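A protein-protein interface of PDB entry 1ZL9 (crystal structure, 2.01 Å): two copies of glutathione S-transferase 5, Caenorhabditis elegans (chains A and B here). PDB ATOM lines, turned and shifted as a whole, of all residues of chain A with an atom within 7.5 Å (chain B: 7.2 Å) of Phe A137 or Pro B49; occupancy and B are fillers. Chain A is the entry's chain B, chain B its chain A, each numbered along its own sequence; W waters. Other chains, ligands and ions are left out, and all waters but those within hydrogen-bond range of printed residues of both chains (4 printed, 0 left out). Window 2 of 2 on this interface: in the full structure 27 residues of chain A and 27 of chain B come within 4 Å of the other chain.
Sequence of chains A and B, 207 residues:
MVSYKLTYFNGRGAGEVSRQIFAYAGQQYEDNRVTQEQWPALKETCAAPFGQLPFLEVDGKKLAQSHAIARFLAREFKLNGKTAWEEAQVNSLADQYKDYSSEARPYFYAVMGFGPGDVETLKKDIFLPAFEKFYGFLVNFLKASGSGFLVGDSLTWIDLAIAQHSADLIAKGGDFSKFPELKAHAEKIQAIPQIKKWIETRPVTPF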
ATOM      1  N   GLN A  89      -1.157 -27.819 -29.267  1.00  0.00           N
ATOM      2  CA  GLN A  89      -2.142 -27.713 -28.176  1.00  0.00           C
ATOM      3  C   GLN A  89      -1.490 -27.274 -26.911  1.00  0.00           C
ATOM      4  O   GLN A  89      -2.084 -26.517 -26.104  1.00  0.00           O
ATOM      5  CB  GLN A  89      -2.838 -29.075 -27.978  1.00  0.00           C
ATOM      6  CG  GLN A  89      -3.726 -29.500 -29.096  1.00  0.00           C
ATOM      7  CD  GLN A  89      -4.916 -28.569 -29.307  1.00  0.00           C
ATOM      8  OE1 GLN A  89      -5.206 -27.740 -28.462  1.00  0.00           O
ATOM      9  NE2 GLN A  89      -5.556 -28.656 -30.459  1.00  0.00           N
ATOM     10  N   SER A  92      -1.181 -23.682 -27.327  1.00  0.00           N
ATOM     11  CA  SER A  92      -2.487 -23.032 -27.195  1.00  0.00           C
ATOM     12  C   SER A  92      -2.814 -22.773 -25.727  1.00  0.00           C
ATOM     13  O   SER A  92      -3.232 -21.676 -25.320  1.00  0.00           O
ATOM     14  CB  SER A  92      -3.550 -23.926 -27.798  1.00  0.00           C
ATOM     15  OG  SER A  92      -4.764 -23.249 -27.930  1.00  0.00           O
ATOM     16  N   LEU A  93      -2.592 -23.801 -24.926  1.00  0.00           N
ATOM     17  CA  LEU A  93      -2.940 -23.733 -23.524  1.00  0.00           C
ATOM     18  C   LEU A  93      -1.993 -22.793 -22.776  1.00  0.00           C
ATOM     19  O   LEU A  93      -2.441 -22.017 -21.957  1.00  0.00           O
ATOM     20  CB  LEU A  93      -2.883 -25.144 -22.926  1.00  0.00           C
ATOM     21  CG  LEU A  93      -3.928 -25.609 -21.912  1.00  0.00           C
ATOM     22  CD1 LEU A  93      -3.348 -26.646 -20.894  1.00  0.00           C
ATOM     23  CD2 LEU A  93      -4.889 -24.583 -21.320  1.00  0.00           C
ATOM     24  N   GLN A  96      -3.075 -19.347 -23.499  1.00  0.00           N
ATOM     25  CA  GLN A  96      -4.259 -19.024 -22.759  1.00  0.00           C
ATOM     26  C   GLN A  96      -3.869 -18.757 -21.266  1.00  0.00           C
ATOM     27  O   GLN A  96      -4.428 -17.880 -20.641  1.00  0.00           O
ATOM     28  CB  GLN A  96      -5.322 -20.127 -22.860  1.00  0.00           C
ATOM     29  CG  GLN A  96      -6.669 -19.729 -22.195  1.00  0.00           C
ATOM     30  CD  GLN A  96      -7.344 -18.562 -22.846  1.00  0.00           C
ATOM     31  OE1 GLN A  96      -7.230 -18.390 -24.073  1.00  0.00           O
ATOM     32  NE2 GLN A  96      -8.098 -17.755 -22.044  1.00  0.00           N
ATOM     33  N   ALA A 130     -11.288 -14.596 -13.277  1.00  0.00           N
ATOM     34  CA  ALA A 130     -10.191 -15.049 -14.128  1.00  0.00           C
ATOM     35  C   ALA A 130      -9.801 -16.497 -13.857  1.00  0.00           C
ATOM     36  O   ALA A 130      -9.646 -17.301 -14.782  1.00  0.00           O
ATOM     37  CB  ALA A 130      -9.004 -14.099 -13.940  1.00  0.00           C
ATOM     38  N   PHE A 131      -9.661 -16.838 -12.583  1.00  0.00           N
ATOM     39  CA  PHE A 131      -9.332 -18.164 -12.157  1.00  0.00           C
ATOM     40  C   PHE A 131     -10.398 -19.144 -12.587  1.00  0.00           C
ATOM     41  O   PHE A 131     -10.079 -20.136 -13.131  1.00  0.00           O
ATOM     42  CB  PHE A 131      -9.205 -18.162 -10.642  1.00  0.00           C
ATOM     43  CG  PHE A 131      -9.034 -19.518 -10.035  1.00  0.00           C
ATOM     44  CD1 PHE A 131      -7.813 -20.145 -10.042  1.00  0.00           C
ATOM     45  CD2 PHE A 131     -10.081 -20.112  -9.361  1.00  0.00           C
ATOM     46  CE1 PHE A 131      -7.651 -21.421  -9.515  1.00  0.00           C
ATOM     47  CE2 PHE A 131      -9.908 -21.349  -8.769  1.00  0.00           C
ATOM     48  CZ  PHE A 131      -8.703 -22.004  -8.867  1.00  0.00           C
ATOM     49  N   GLU A 132     -11.677 -18.794 -12.432  1.00  0.00           N
ATOM     50  CA  GLU A 132     -12.772 -19.735 -12.734  1.00  0.00           C
ATOM     51  C   GLU A 132     -12.901 -20.008 -14.243  1.00  0.00           C
ATOM     52  O   GLU A 132     -13.065 -21.169 -14.678  1.00  0.00           O
ATOM     53  CB  GLU A 132     -14.079 -19.271 -12.083  1.00  0.00           C
ATOM     54  CG  GLU A 132     -13.956 -19.480 -10.566  1.00  0.00           C
ATOM     55  CD  GLU A 132     -15.228 -19.136  -9.775  1.00  0.00           C
ATOM     56  OE1 GLU A 132     -16.171 -18.618 -10.370  1.00  0.00           O
ATOM     57  OE2 GLU A 132     -15.218 -19.322  -8.519  1.00  0.00           O
ATOM     58  N   LYS A 133     -12.709 -18.960 -15.020  1.00  0.00           N
ATOM     59  CA  LYS A 133     -12.698 -19.111 -16.479  1.00  0.00           C
ATOM     60  C   LYS A 133     -11.559 -19.985 -16.949  1.00  0.00           C
ATOM     61  O   LYS A 133     -11.763 -20.942 -17.708  1.00  0.00           O
ATOM     62  CB  LYS A 133     -12.748 -17.743 -17.174  1.00  0.00           C
ATOM     63  CG  LYS A 133     -12.455 -17.797 -18.665  1.00  0.00           C
ATOM     64  CD  LYS A 133     -12.794 -16.464 -19.420  1.00  0.00           C
ATOM     65  CE  LYS A 133     -11.579 -15.824 -20.143  1.00  0.00           C
ATOM     66  NZ  LYS A 133     -11.404 -14.291 -19.827  1.00  0.00           N
ATOM     67  N   PHE A 134     -10.359 -19.705 -16.466  1.00  0.00           N
ATOM     68  CA  PHE A 134      -9.164 -20.393 -16.960  1.00  0.00           C
ATOM     69  C   PHE A 134      -9.137 -21.858 -16.467  1.00  0.00           C
ATOM     70  O   PHE A 134      -8.861 -22.798 -17.227  1.00  0.00           O
ATOM     71  CB  PHE A 134      -7.870 -19.666 -16.515  1.00  0.00           C
ATOM     72  CG  PHE A 134      -6.625 -20.363 -16.988  1.00  0.00           C
ATOM     73  CD1 PHE A 134      -5.688 -20.837 -16.108  1.00  0.00           C
ATOM     74  CD2 PHE A 134      -6.474 -20.668 -18.337  1.00  0.00           C
ATOM     75  CE1 PHE A 134      -4.582 -21.557 -16.570  1.00  0.00           C
ATOM     76  CE2 PHE A 134      -5.362 -21.384 -18.787  1.00  0.00           C
ATOM     77  CZ  PHE A 134      -4.430 -21.828 -17.882  1.00  0.00           C
ATOM     78  N   TYR A 135      -9.471 -22.046 -15.194  1.00  0.00           N
ATOM     79  CA  TYR A 135      -9.489 -23.396 -14.654  1.00  0.00           C
ATOM     80  C   TYR A 135     -10.575 -24.265 -15.255  1.00  0.00           C
ATOM     81  O   TYR A 135     -10.398 -25.479 -15.357  1.00  0.00           O
ATOM     82  CB  TYR A 135      -9.423 -23.387 -13.113  1.00  0.00           C
ATOM     83  CG  TYR A 135      -7.995 -23.325 -12.625  1.00  0.00           C
ATOM     84  CD1 TYR A 135      -7.139 -22.198 -12.914  1.00  0.00           C
ATOM     85  CD2 TYR A 135      -7.450 -24.377 -11.945  1.00  0.00           C
ATOM     86  CE1 TYR A 135      -5.793 -22.199 -12.509  1.00  0.00           C
ATOM     87  CE2 TYR A 135      -6.132 -24.391 -11.535  1.00  0.00           C
ATOM     88  CZ  TYR A 135      -5.295 -23.306 -11.807  1.00  0.00           C
ATOM     89  OH  TYR A 135      -3.987 -23.376 -11.409  1.00  0.00           O
ATOM     90  N   GLY A 136     -11.682 -23.667 -15.707  1.00  0.00           N
ATOM     91  CA  GLY A 136     -12.712 -24.407 -16.434  1.00  0.00           C
ATOM     92  C   GLY A 136     -12.156 -24.973 -17.719  1.00  0.00           C
ATOM     93  O   GLY A 136     -12.394 -26.157 -18.111  1.00  0.00           O
ATOM     94  N   PHE A 137     -11.285 -24.184 -18.360  1.00  0.00           N
ATOM     95  CA  PHE A 137     -10.611 -24.642 -19.591  1.00  0.00           C
ATOM     96  C   PHE A 137      -9.617 -25.727 -19.292  1.00  0.00           C
ATOM     97  O   PHE A 137      -9.535 -26.721 -20.033  1.00  0.00           O
ATOM     98  CB  PHE A 137      -9.929 -23.509 -20.329  1.00  0.00           C
ATOM     99  CG  PHE A 137     -10.828 -22.396 -20.746  1.00  0.00           C
ATOM    100  CD1 PHE A 137     -10.324 -21.059 -20.754  1.00  0.00           C
ATOM    101  CD2 PHE A 137     -12.103 -22.622 -21.253  1.00  0.00           C
ATOM    102  CE1 PHE A 137     -11.110 -19.988 -21.248  1.00  0.00           C
ATOM    103  CE2 PHE A 137     -12.911 -21.514 -21.694  1.00  0.00           C
ATOM    104  CZ  PHE A 137     -12.420 -20.220 -21.668  1.00  0.00           C
ATOM    105  N   LEU A 138      -8.876 -25.610 -18.198  1.00  0.00           N
ATOM    106  CA  LEU A 138      -7.927 -26.680 -17.793  1.00  0.00           C
ATOM    107  C   LEU A 138      -8.669 -28.008 -17.658  1.00  0.00           C
ATOM    108  O   LEU A 138      -8.153 -29.088 -18.020  1.00  0.00           O
ATOM    109  CB  LEU A 138      -7.202 -26.337 -16.483  1.00  0.00           C
ATOM    110  CG  LEU A 138      -6.200 -25.168 -16.547  1.00  0.00           C
ATOM    111  CD1 LEU A 138      -5.628 -24.881 -15.173  1.00  0.00           C
ATOM    112  CD2 LEU A 138      -5.054 -25.507 -17.475  1.00  0.00           C
ATOM    113  N   VAL A 139      -9.848 -27.950 -17.041  1.00  0.00           N
ATOM    114  CA  VAL A 139     -10.616 -29.170 -16.795  1.00  0.00           C
ATOM    115  C   VAL A 139     -11.045 -29.750 -18.138  1.00  0.00           C
ATOM    116  O   VAL A 139     -11.035 -30.952 -18.347  1.00  0.00           O
ATOM    117  CB  VAL A 139     -11.893 -28.882 -15.910  1.00  0.00           C
ATOM    118  CG1 VAL A 139     -12.823 -30.061 -15.916  1.00  0.00           C
ATOM    119  CG2 VAL A 139     -11.487 -28.541 -14.435  1.00  0.00           C
ATOM    120  N   ASN A 140     -11.454 -28.907 -19.064  1.00  0.00           N
ATOM    121  CA  ASN A 140     -11.744 -29.352 -20.443  1.00  0.00           C
ATOM    122  C   ASN A 140     -10.569 -30.147 -21.077  1.00  0.00           C
ATOM    123  O   ASN A 140     -10.749 -31.205 -21.674  1.00  0.00           O
ATOM    124  CB  ASN A 140     -12.075 -28.190 -21.389  1.00  0.00           C
ATOM    125  CG  ASN A 140     -13.369 -27.503 -21.072  1.00  0.00           C
ATOM    126  OD1 ASN A 140     -14.182 -28.032 -20.334  1.00  0.00           O
ATOM    127  ND2 ASN A 140     -13.548 -26.268 -21.602  1.00  0.00           N
ATOM    128  N   PHE A 141      -9.371 -29.627 -20.966  1.00  0.00           N
ATOM    129  CA  PHE A 141      -8.190 -30.328 -21.482  1.00  0.00           C
ATOM    130  C   PHE A 141      -7.927 -31.669 -20.758  1.00  0.00           C
ATOM    131  O   PHE A 141      -7.594 -32.653 -21.411  1.00  0.00           O
ATOM    132  CB  PHE A 141      -6.969 -29.423 -21.356  1.00  0.00           C
ATOM    133  CG  PHE A 141      -6.776 -28.539 -22.576  1.00  0.00           C
ATOM    134  CD1 PHE A 141      -7.707 -27.555 -22.904  1.00  0.00           C
ATOM    135  CD2 PHE A 141      -5.705 -28.746 -23.427  1.00  0.00           C
ATOM    136  CE1 PHE A 141      -7.567 -26.773 -24.049  1.00  0.00           C
ATOM    137  CE2 PHE A 141      -5.557 -27.948 -24.567  1.00  0.00           C
ATOM    138  CZ  PHE A 141      -6.477 -26.982 -24.874  1.00  0.00           C
ATOM    139  N   LEU A 142      -8.063 -31.700 -19.432  1.00  0.00           N
ATOM    140  CA  LEU A 142      -7.896 -32.929 -18.695  1.00  0.00           C
ATOM    141  C   LEU A 142      -8.875 -33.961 -19.172  1.00  0.00           C
ATOM    142  O   LEU A 142      -8.486 -35.079 -19.403  1.00  0.00           O
ATOM    143  CB  LEU A 142      -8.018 -32.756 -17.187  1.00  0.00           C
ATOM    144  CG  LEU A 142      -6.910 -31.975 -16.519  1.00  0.00           C
ATOM    145  CD1 LEU A 142      -7.343 -31.755 -15.046  1.00  0.00           C
ATOM    146  CD2 LEU A 142      -5.630 -32.732 -16.572  1.00  0.00           C
ATOM    147  N   LYS A 143     -10.122 -33.569 -19.358  1.00  0.00           N
ATOM    148  CA  LYS A 143     -11.133 -34.511 -19.773  1.00  0.00           C
ATOM    149  C   LYS A 143     -10.881 -34.990 -21.192  1.00  0.00           C
ATOM    150  O   LYS A 143     -11.024 -36.171 -21.485  1.00  0.00           O
ATOM    151  CB  LYS A 143     -12.533 -33.931 -19.628  1.00  0.00           C
ATOM    152  CG  LYS A 143     -12.903 -33.583 -18.183  1.00  0.00           C
ATOM    153  CD  LYS A 143     -14.370 -33.144 -18.060  1.00  0.00           C
ATOM    154  CE  LYS A 143     -14.777 -33.004 -16.565  1.00  0.00           C
ATOM    155  NZ  LYS A 143     -16.052 -32.162 -16.449  1.00  0.00           N
ATOM    156  N   LEU A 150      -2.412 -32.753 -19.141  1.00  0.00           N
ATOM    157  CA  LEU A 150      -3.214 -31.746 -19.822  1.00  0.00           C
ATOM    158  C   LEU A 150      -3.267 -32.005 -21.309  1.00  0.00           C
ATOM    159  O   LEU A 150      -4.243 -31.725 -21.942  1.00  0.00           O
ATOM    160  CB  LEU A 150      -2.672 -30.319 -19.556  1.00  0.00           C
ATOM    161  CG  LEU A 150      -2.995 -29.868 -18.142  1.00  0.00           C
ATOM    162  CD1 LEU A 150      -2.089 -28.720 -17.640  1.00  0.00           C
ATOM    163  CD2 LEU A 150      -4.455 -29.454 -18.070  1.00  0.00           C
ATOM    164  N   PHE A 179     -12.753 -27.074  -8.829  1.00  0.00           N
ATOM    165  CA  PHE A 179     -11.776 -27.740  -9.707  1.00  0.00           C
ATOM    166  C   PHE A 179     -10.958 -28.789  -9.029  1.00  0.00           C
ATOM    167  O   PHE A 179      -9.742 -28.777  -9.106  1.00  0.00           O
ATOM    168  CB  PHE A 179     -10.852 -26.654 -10.320  1.00  0.00           C
ATOM    169  CG  PHE A 179     -11.615 -25.517 -10.900  1.00  0.00           C
ATOM    170  CD1 PHE A 179     -11.598 -24.262 -10.316  1.00  0.00           C
ATOM    171  CD2 PHE A 179     -12.396 -25.717 -12.011  1.00  0.00           C
ATOM    172  CE1 PHE A 179     -12.344 -23.248 -10.874  1.00  0.00           C
ATOM    173  CE2 PHE A 179     -13.121 -24.716 -12.561  1.00  0.00           C
ATOM    174  CZ  PHE A 179     -13.104 -23.471 -11.990  1.00  0.00           C
ATOM    175  N   LEU A 182      -7.855 -30.265 -10.675  1.00  0.00           N
ATOM    176  CA  LEU A 182      -6.572 -29.584 -10.725  1.00  0.00           C
ATOM    177  C   LEU A 182      -5.760 -29.696  -9.481  1.00  0.00           C
ATOM    178  O   LEU A 182      -4.507 -29.549  -9.501  1.00  0.00           O
ATOM    179  CB  LEU A 182      -6.736 -28.141 -11.174  1.00  0.00           C
ATOM    180  CG  LEU A 182      -6.764 -27.885 -12.706  1.00  0.00           C
ATOM    181  CD1 LEU A 182      -5.521 -28.355 -13.467  1.00  0.00           C
ATOM    182  CD2 LEU A 182      -8.013 -28.383 -13.402  1.00  0.00           C
ATOM    183  N   CYS B  46     -19.992 -23.052 -27.568  1.00  0.00           N
ATOM    184  CA  CYS B  46     -18.634 -23.489 -27.251  1.00  0.00           C
ATOM    185  C   CYS B  46     -17.943 -23.996 -28.501  1.00  0.00           C
ATOM    186  O   CYS B  46     -17.268 -25.021 -28.461  1.00  0.00           O
ATOM    187  CB  CYS B  46     -18.614 -24.574 -26.158  1.00  0.00           C
ATOM    188  SG  CYS B  46     -19.552 -24.141 -24.648  1.00  0.00           S
ATOM    189  N   ALA B  47     -18.103 -23.318 -29.634  1.00  0.00           N
ATOM    190  CA  ALA B  47     -17.314 -23.745 -30.780  1.00  0.00           C
ATOM    191  C   ALA B  47     -15.844 -23.495 -30.376  1.00  0.00           C
ATOM    192  O   ALA B  47     -15.058 -24.423 -30.296  1.00  0.00           O
ATOM    193  CB  ALA B  47     -17.708 -23.019 -32.073  1.00  0.00           C
ATOM    194  N   ALA B  48     -15.507 -22.274 -30.005  1.00  0.00           N
ATOM    195  CA  ALA B  48     -14.106 -21.926 -29.807  1.00  0.00           C
ATOM    196  C   ALA B  48     -13.558 -22.530 -28.507  1.00  0.00           C
ATOM    197  O   ALA B  48     -14.175 -22.373 -27.465  1.00  0.00           O
ATOM    198  CB  ALA B  48     -13.971 -20.403 -29.820  1.00  0.00           C
ATOM    199  N   PRO B  49     -12.413 -23.196 -28.553  1.00  0.00           N
ATOM    200  CA  PRO B  49     -11.806 -23.781 -27.349  1.00  0.00           C
ATOM    201  C   PRO B  49     -11.765 -22.877 -26.120  1.00  0.00           C
ATOM    202  O   PRO B  49     -12.041 -23.335 -25.003  1.00  0.00           O
ATOM    203  CB  PRO B  49     -10.385 -24.125 -27.814  1.00  0.00           C
ATOM    204  CG  PRO B  49     -10.594 -24.508 -29.250  1.00  0.00           C
ATOM    205  CD  PRO B  49     -11.603 -23.504 -29.753  1.00  0.00           C
ATOM    206  N   PHE B  50     -11.429 -21.615 -26.323  1.00  0.00           N
ATOM    207  CA  PHE B  50     -11.431 -20.655 -25.242  1.00  0.00           C
ATOM    208  C   PHE B  50     -12.419 -19.542 -25.422  1.00  0.00           C
ATOM    209  O   PHE B  50     -12.246 -18.449 -24.860  1.00  0.00           O
ATOM    210  CB  PHE B  50     -10.038 -20.073 -25.025  1.00  0.00           C
ATOM    211  CG  PHE B  50      -8.988 -21.109 -24.902  1.00  0.00           C
ATOM    212  CD1 PHE B  50      -7.856 -21.059 -25.727  1.00  0.00           C
ATOM    213  CD2 PHE B  50      -9.119 -22.162 -24.002  1.00  0.00           C
ATOM    214  CE1 PHE B  50      -6.850 -21.999 -25.625  1.00  0.00           C
ATOM    215  CE2 PHE B  50      -8.076 -23.154 -23.881  1.00  0.00           C
ATOM    216  CZ  PHE B  50      -6.964 -23.080 -24.729  1.00  0.00           C
ATOM    217  N   GLY B  51     -13.452 -19.797 -26.189  1.00  0.00           N
ATOM    218  CA  GLY B  51     -14.522 -18.812 -26.363  1.00  0.00           C
ATOM    219  C   GLY B  51     -14.141 -17.627 -27.238  1.00  0.00           C
ATOM    220  O   GLY B  51     -14.838 -16.589 -27.226  1.00  0.00           O
ATOM    221  N   GLN B  52     -13.010 -17.703 -27.929  1.00  0.00           N
ATOM    222  CA  GLN B  52     -12.519 -16.528 -28.666  1.00  0.00           C
ATOM    223  C   GLN B  52     -11.988 -16.938 -30.052  1.00  0.00           C
ATOM    224  O   GLN B  52     -11.730 -18.133 -30.265  1.00  0.00           O
ATOM    225  CB  GLN B  52     -11.397 -15.813 -27.878  1.00  0.00           C
ATOM    226  CG  GLN B  52     -11.959 -15.179 -26.582  1.00  0.00           C
ATOM    227  CD  GLN B  52     -11.053 -14.176 -25.997  1.00  0.00           C
ATOM    228  OE1 GLN B  52     -11.396 -12.975 -25.930  1.00  0.00           O
ATOM    229  NE2 GLN B  52      -9.880 -14.626 -25.568  1.00  0.00           N
ATOM    230  N   PRO B  54      -8.942 -15.989 -33.143  1.00  0.00           N
ATOM    231  CA  PRO B  54      -9.178 -17.080 -34.103  1.00  0.00           C
ATOM    232  C   PRO B  54      -9.109 -18.496 -33.567  1.00  0.00           C
ATOM    233  O   PRO B  54      -8.599 -18.739 -32.466  1.00  0.00           O
ATOM    234  CB  PRO B  54      -8.010 -16.883 -35.098  1.00  0.00           C
ATOM    235  CG  PRO B  54      -6.899 -16.370 -34.217  1.00  0.00           C
ATOM    236  CD  PRO B  54      -7.565 -15.475 -33.246  1.00  0.00           C
ATOM    237  N   PHE B  55      -9.670 -19.433 -34.322  1.00  0.00           N
ATOM    238  CA  PHE B  55      -9.335 -20.830 -34.154  1.00  0.00           C
ATOM    239  C   PHE B  55      -9.279 -21.481 -35.510  1.00  0.00           C
ATOM    240  O   PHE B  55      -9.869 -20.990 -36.474  1.00  0.00           O
ATOM    241  CB  PHE B  55     -10.247 -21.574 -33.151  1.00  0.00           C
ATOM    242  CG  PHE B  55     -11.656 -21.769 -33.621  1.00  0.00           C
ATOM    243  CD1 PHE B  55     -12.003 -22.858 -34.404  1.00  0.00           C
ATOM    244  CD2 PHE B  55     -12.623 -20.862 -33.289  1.00  0.00           C
ATOM    245  CE1 PHE B  55     -13.353 -23.036 -34.827  1.00  0.00           C
ATOM    246  CE2 PHE B  55     -13.941 -21.033 -33.658  1.00  0.00           C
ATOM    247  CZ  PHE B  55     -14.321 -22.129 -34.420  1.00  0.00           C
ATOM    248  N   LEU B  56      -8.463 -22.523 -35.593  1.00  0.00           N
ATOM    249  CA  LEU B  56      -8.213 -23.226 -36.827  1.00  0.00           C
ATOM    250  C   LEU B  56      -8.774 -24.627 -36.652  1.00  0.00           C
ATOM    251  O   LEU B  56      -8.608 -25.226 -35.604  1.00  0.00           O
ATOM    252  CB  LEU B  56      -6.724 -23.333 -37.090  1.00  0.00           C
ATOM    253  CG  LEU B  56      -6.278 -24.202 -38.242  1.00  0.00           C
ATOM    254  CD1 LEU B  56      -6.526 -23.432 -39.525  1.00  0.00           C
ATOM    255  CD2 LEU B  56      -4.816 -24.633 -38.150  1.00  0.00           C
ATOM    256  N   LYS B  62      -9.991 -28.742 -33.439  1.00  0.00           N
ATOM    257  CA  LYS B  62      -9.863 -27.308 -33.193  1.00  0.00           C
ATOM    258  C   LYS B  62      -8.516 -26.947 -32.549  1.00  0.00           C
ATOM    259  O   LYS B  62      -8.025 -27.629 -31.641  1.00  0.00           O
ATOM    260  CB  LYS B  62     -11.026 -26.779 -32.332  1.00  0.00           C
ATOM    261  CG  LYS B  62     -12.346 -26.696 -33.154  1.00  0.00           C
ATOM    262  CD  LYS B  62     -13.521 -26.410 -32.275  1.00  0.00           C
ATOM    263  CE  LYS B  62     -14.839 -27.009 -32.854  1.00  0.00           C
ATOM    264  NZ  LYS B  62     -15.661 -25.877 -33.334  1.00  0.00           N
ATOM    265  N   LEU B  63      -7.972 -25.800 -32.976  1.00  0.00           N
ATOM    266  CA  LEU B  63      -6.774 -25.247 -32.361  1.00  0.00           C
ATOM    267  C   LEU B  63      -6.983 -23.750 -32.226  1.00  0.00           C
ATOM    268  O   LEU B  63      -7.144 -23.061 -33.205  1.00  0.00           O
ATOM    269  CB  LEU B  63      -5.559 -25.515 -33.233  1.00  0.00           C
ATOM    270  CG  LEU B  63      -4.241 -24.858 -32.753  1.00  0.00           C
ATOM    271  CD1 LEU B  63      -3.832 -25.418 -31.420  1.00  0.00           C
ATOM    272  CD2 LEU B  63      -3.198 -25.013 -33.801  1.00  0.00           C
ATOM    273  N   ALA B  64      -6.939 -23.258 -30.997  1.00  0.00           N
ATOM    274  CA  ALA B  64      -7.066 -21.850 -30.677  1.00  0.00           C
ATOM    275  C   ALA B  64      -5.721 -21.198 -30.447  1.00  0.00           C
ATOM    276  O   ALA B  64      -4.688 -21.885 -30.341  1.00  0.00           O
ATOM    277  CB  ALA B  64      -7.838 -21.773 -29.403  1.00  0.00           C
ATOM    278  N   GLN B  65      -5.780 -19.879 -30.266  1.00  0.00           N
ATOM    279  CA  GLN B  65      -4.655 -18.979 -29.940  1.00  0.00           C
ATOM    280  C   GLN B  65      -3.805 -18.587 -31.167  1.00  0.00           C
ATOM    281  O   GLN B  65      -3.149 -19.432 -31.760  1.00  0.00           O
ATOM    282  CB  GLN B  65      -3.804 -19.521 -28.805  1.00  0.00           C
ATOM    283  CG  GLN B  65      -4.544 -19.342 -27.428  1.00  0.00           C
ATOM    284  CD  GLN B  65      -4.453 -17.953 -26.834  1.00  0.00           C
ATOM    285  OE1 GLN B  65      -5.116 -17.643 -25.809  1.00  0.00           O
ATOM    286  NE2 GLN B  65      -3.647 -17.128 -27.412  1.00  0.00           N
HETATM  287  O   HOH W   1      -8.147 -16.617 -26.020  1.00  0.00           O
HETATM  288  O   HOH W   2      -6.667 -25.160 -28.744  1.00  0.00           O
HETATM  289  O   HOH W   3     -10.670 -16.657 -23.449  1.00  0.00           O
HETATM  290  O   HOH W   4     -11.415 -25.583 -23.538  1.00  0.00           O
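O of Ala B47 lies close to NZ of Lys B62, 3.4 Å away. The backbone carbonyl oxygen (O) of Leu B56 lies within hydrogen-bond range of the backbone NH (N) of Leu B63 (2.8 Å).
NE2 of Gln A89 touches CD1 of Leu B63 (3.8 Å). Ser A92 touches Phe B50 (OG to CE1, 3.4 Å). CB of Ser A92 touches CD1 of Leu B63, 3.9 Å away. Ser A92 touches Gln B65. OE1 of Gln A96 touches CD1 of Phe B50, 3.2 Å away. Phe A137 touches Pro B49. Phe A137 touches Phe B50 (CD1 to CD2, 3.6 Å). CE2 of Phe B50 touches CE1 of Phe A141, 3.7 Å away.
The side-chain amide nitrogen (NE2) of Gln A89 is in hydrogen-bond range of the backbone carbonyl oxygen (O) of Lys B62 (2.9 Å). The side-chain hydroxyl (OG) of Ser A92 is in hydrogen-bond range of the backbone carbonyl oxygen (O) of Ala B64, at 2.8 Å. The side-chain amide oxygen (OE1) of Gln B65 lies close to the side-chain amide oxygen (OE1) of Gln A96.
Water W1 lies within hydrogen-bond range of the side-chain amide nitrogen (NE2) of Gln B52, the side-chain amide oxygen (OE1) of Gln A96 and the side-chain amide oxygen (OE1) of Gln B65. Water W4 lies within hydrogen-bond range of O of Pro B49 and ND2 of Asn A140. Water W3 lies within hydrogen-bond range of the backbone carbonyl oxygen of Phe B50 (2.8 Å), the side-chain amide nitrogen of Gln B52 (3.0 Å) and the side-chain amide nitrogen of Gln A96 (3.1 Å). Water W2 lies within hydrogen-bond range of the side-chain hydroxyl (OG) of Ser A92 (2.8 Å), the backbone NH (N) of Ala B64 (3.0 Å) and the side-chain amide oxygen (OE1) of Gln A89 (3.0 Å).
Hydrophobic or aromatic side chains of chain A within 4 Å of the printed part of chain B: Phe A137 and Phe A141. Printed residues of chain B that touch a printed residue of chain A: Pro B49, Phe B50, Lys B62, Leu B63, Ala B64 and Gln B65. Hydrophobic or aromatic side chains of chain B that line the printed part of chain A: Phe B50, Leu B63 and Ala B64. Among the printed residues, 11 pairs touch across the chains.
No position is printed for both chains. Of the 11 pairs that touch across the chains among the printed residues, none has its exchanged pair printed and touching as well.
Phe A137 touches two residues of chain B. Leu A138 touches none of the printed residues of chain B. Pro B49 touches one residue of chain A. Of the printed residues of chain A, Phe B50 touches Ser A92 (3.4 Å), Gln A96 (3.2 Å), Phe A137 (3.6 Å) and Phe A141 (3.7 Å). Printed residues of chain A within 4 Å of Ala B64: Ser A92. The nearest printed residue of chain A that does not touch Phe B50 is Leu A93 (4.3 Å).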
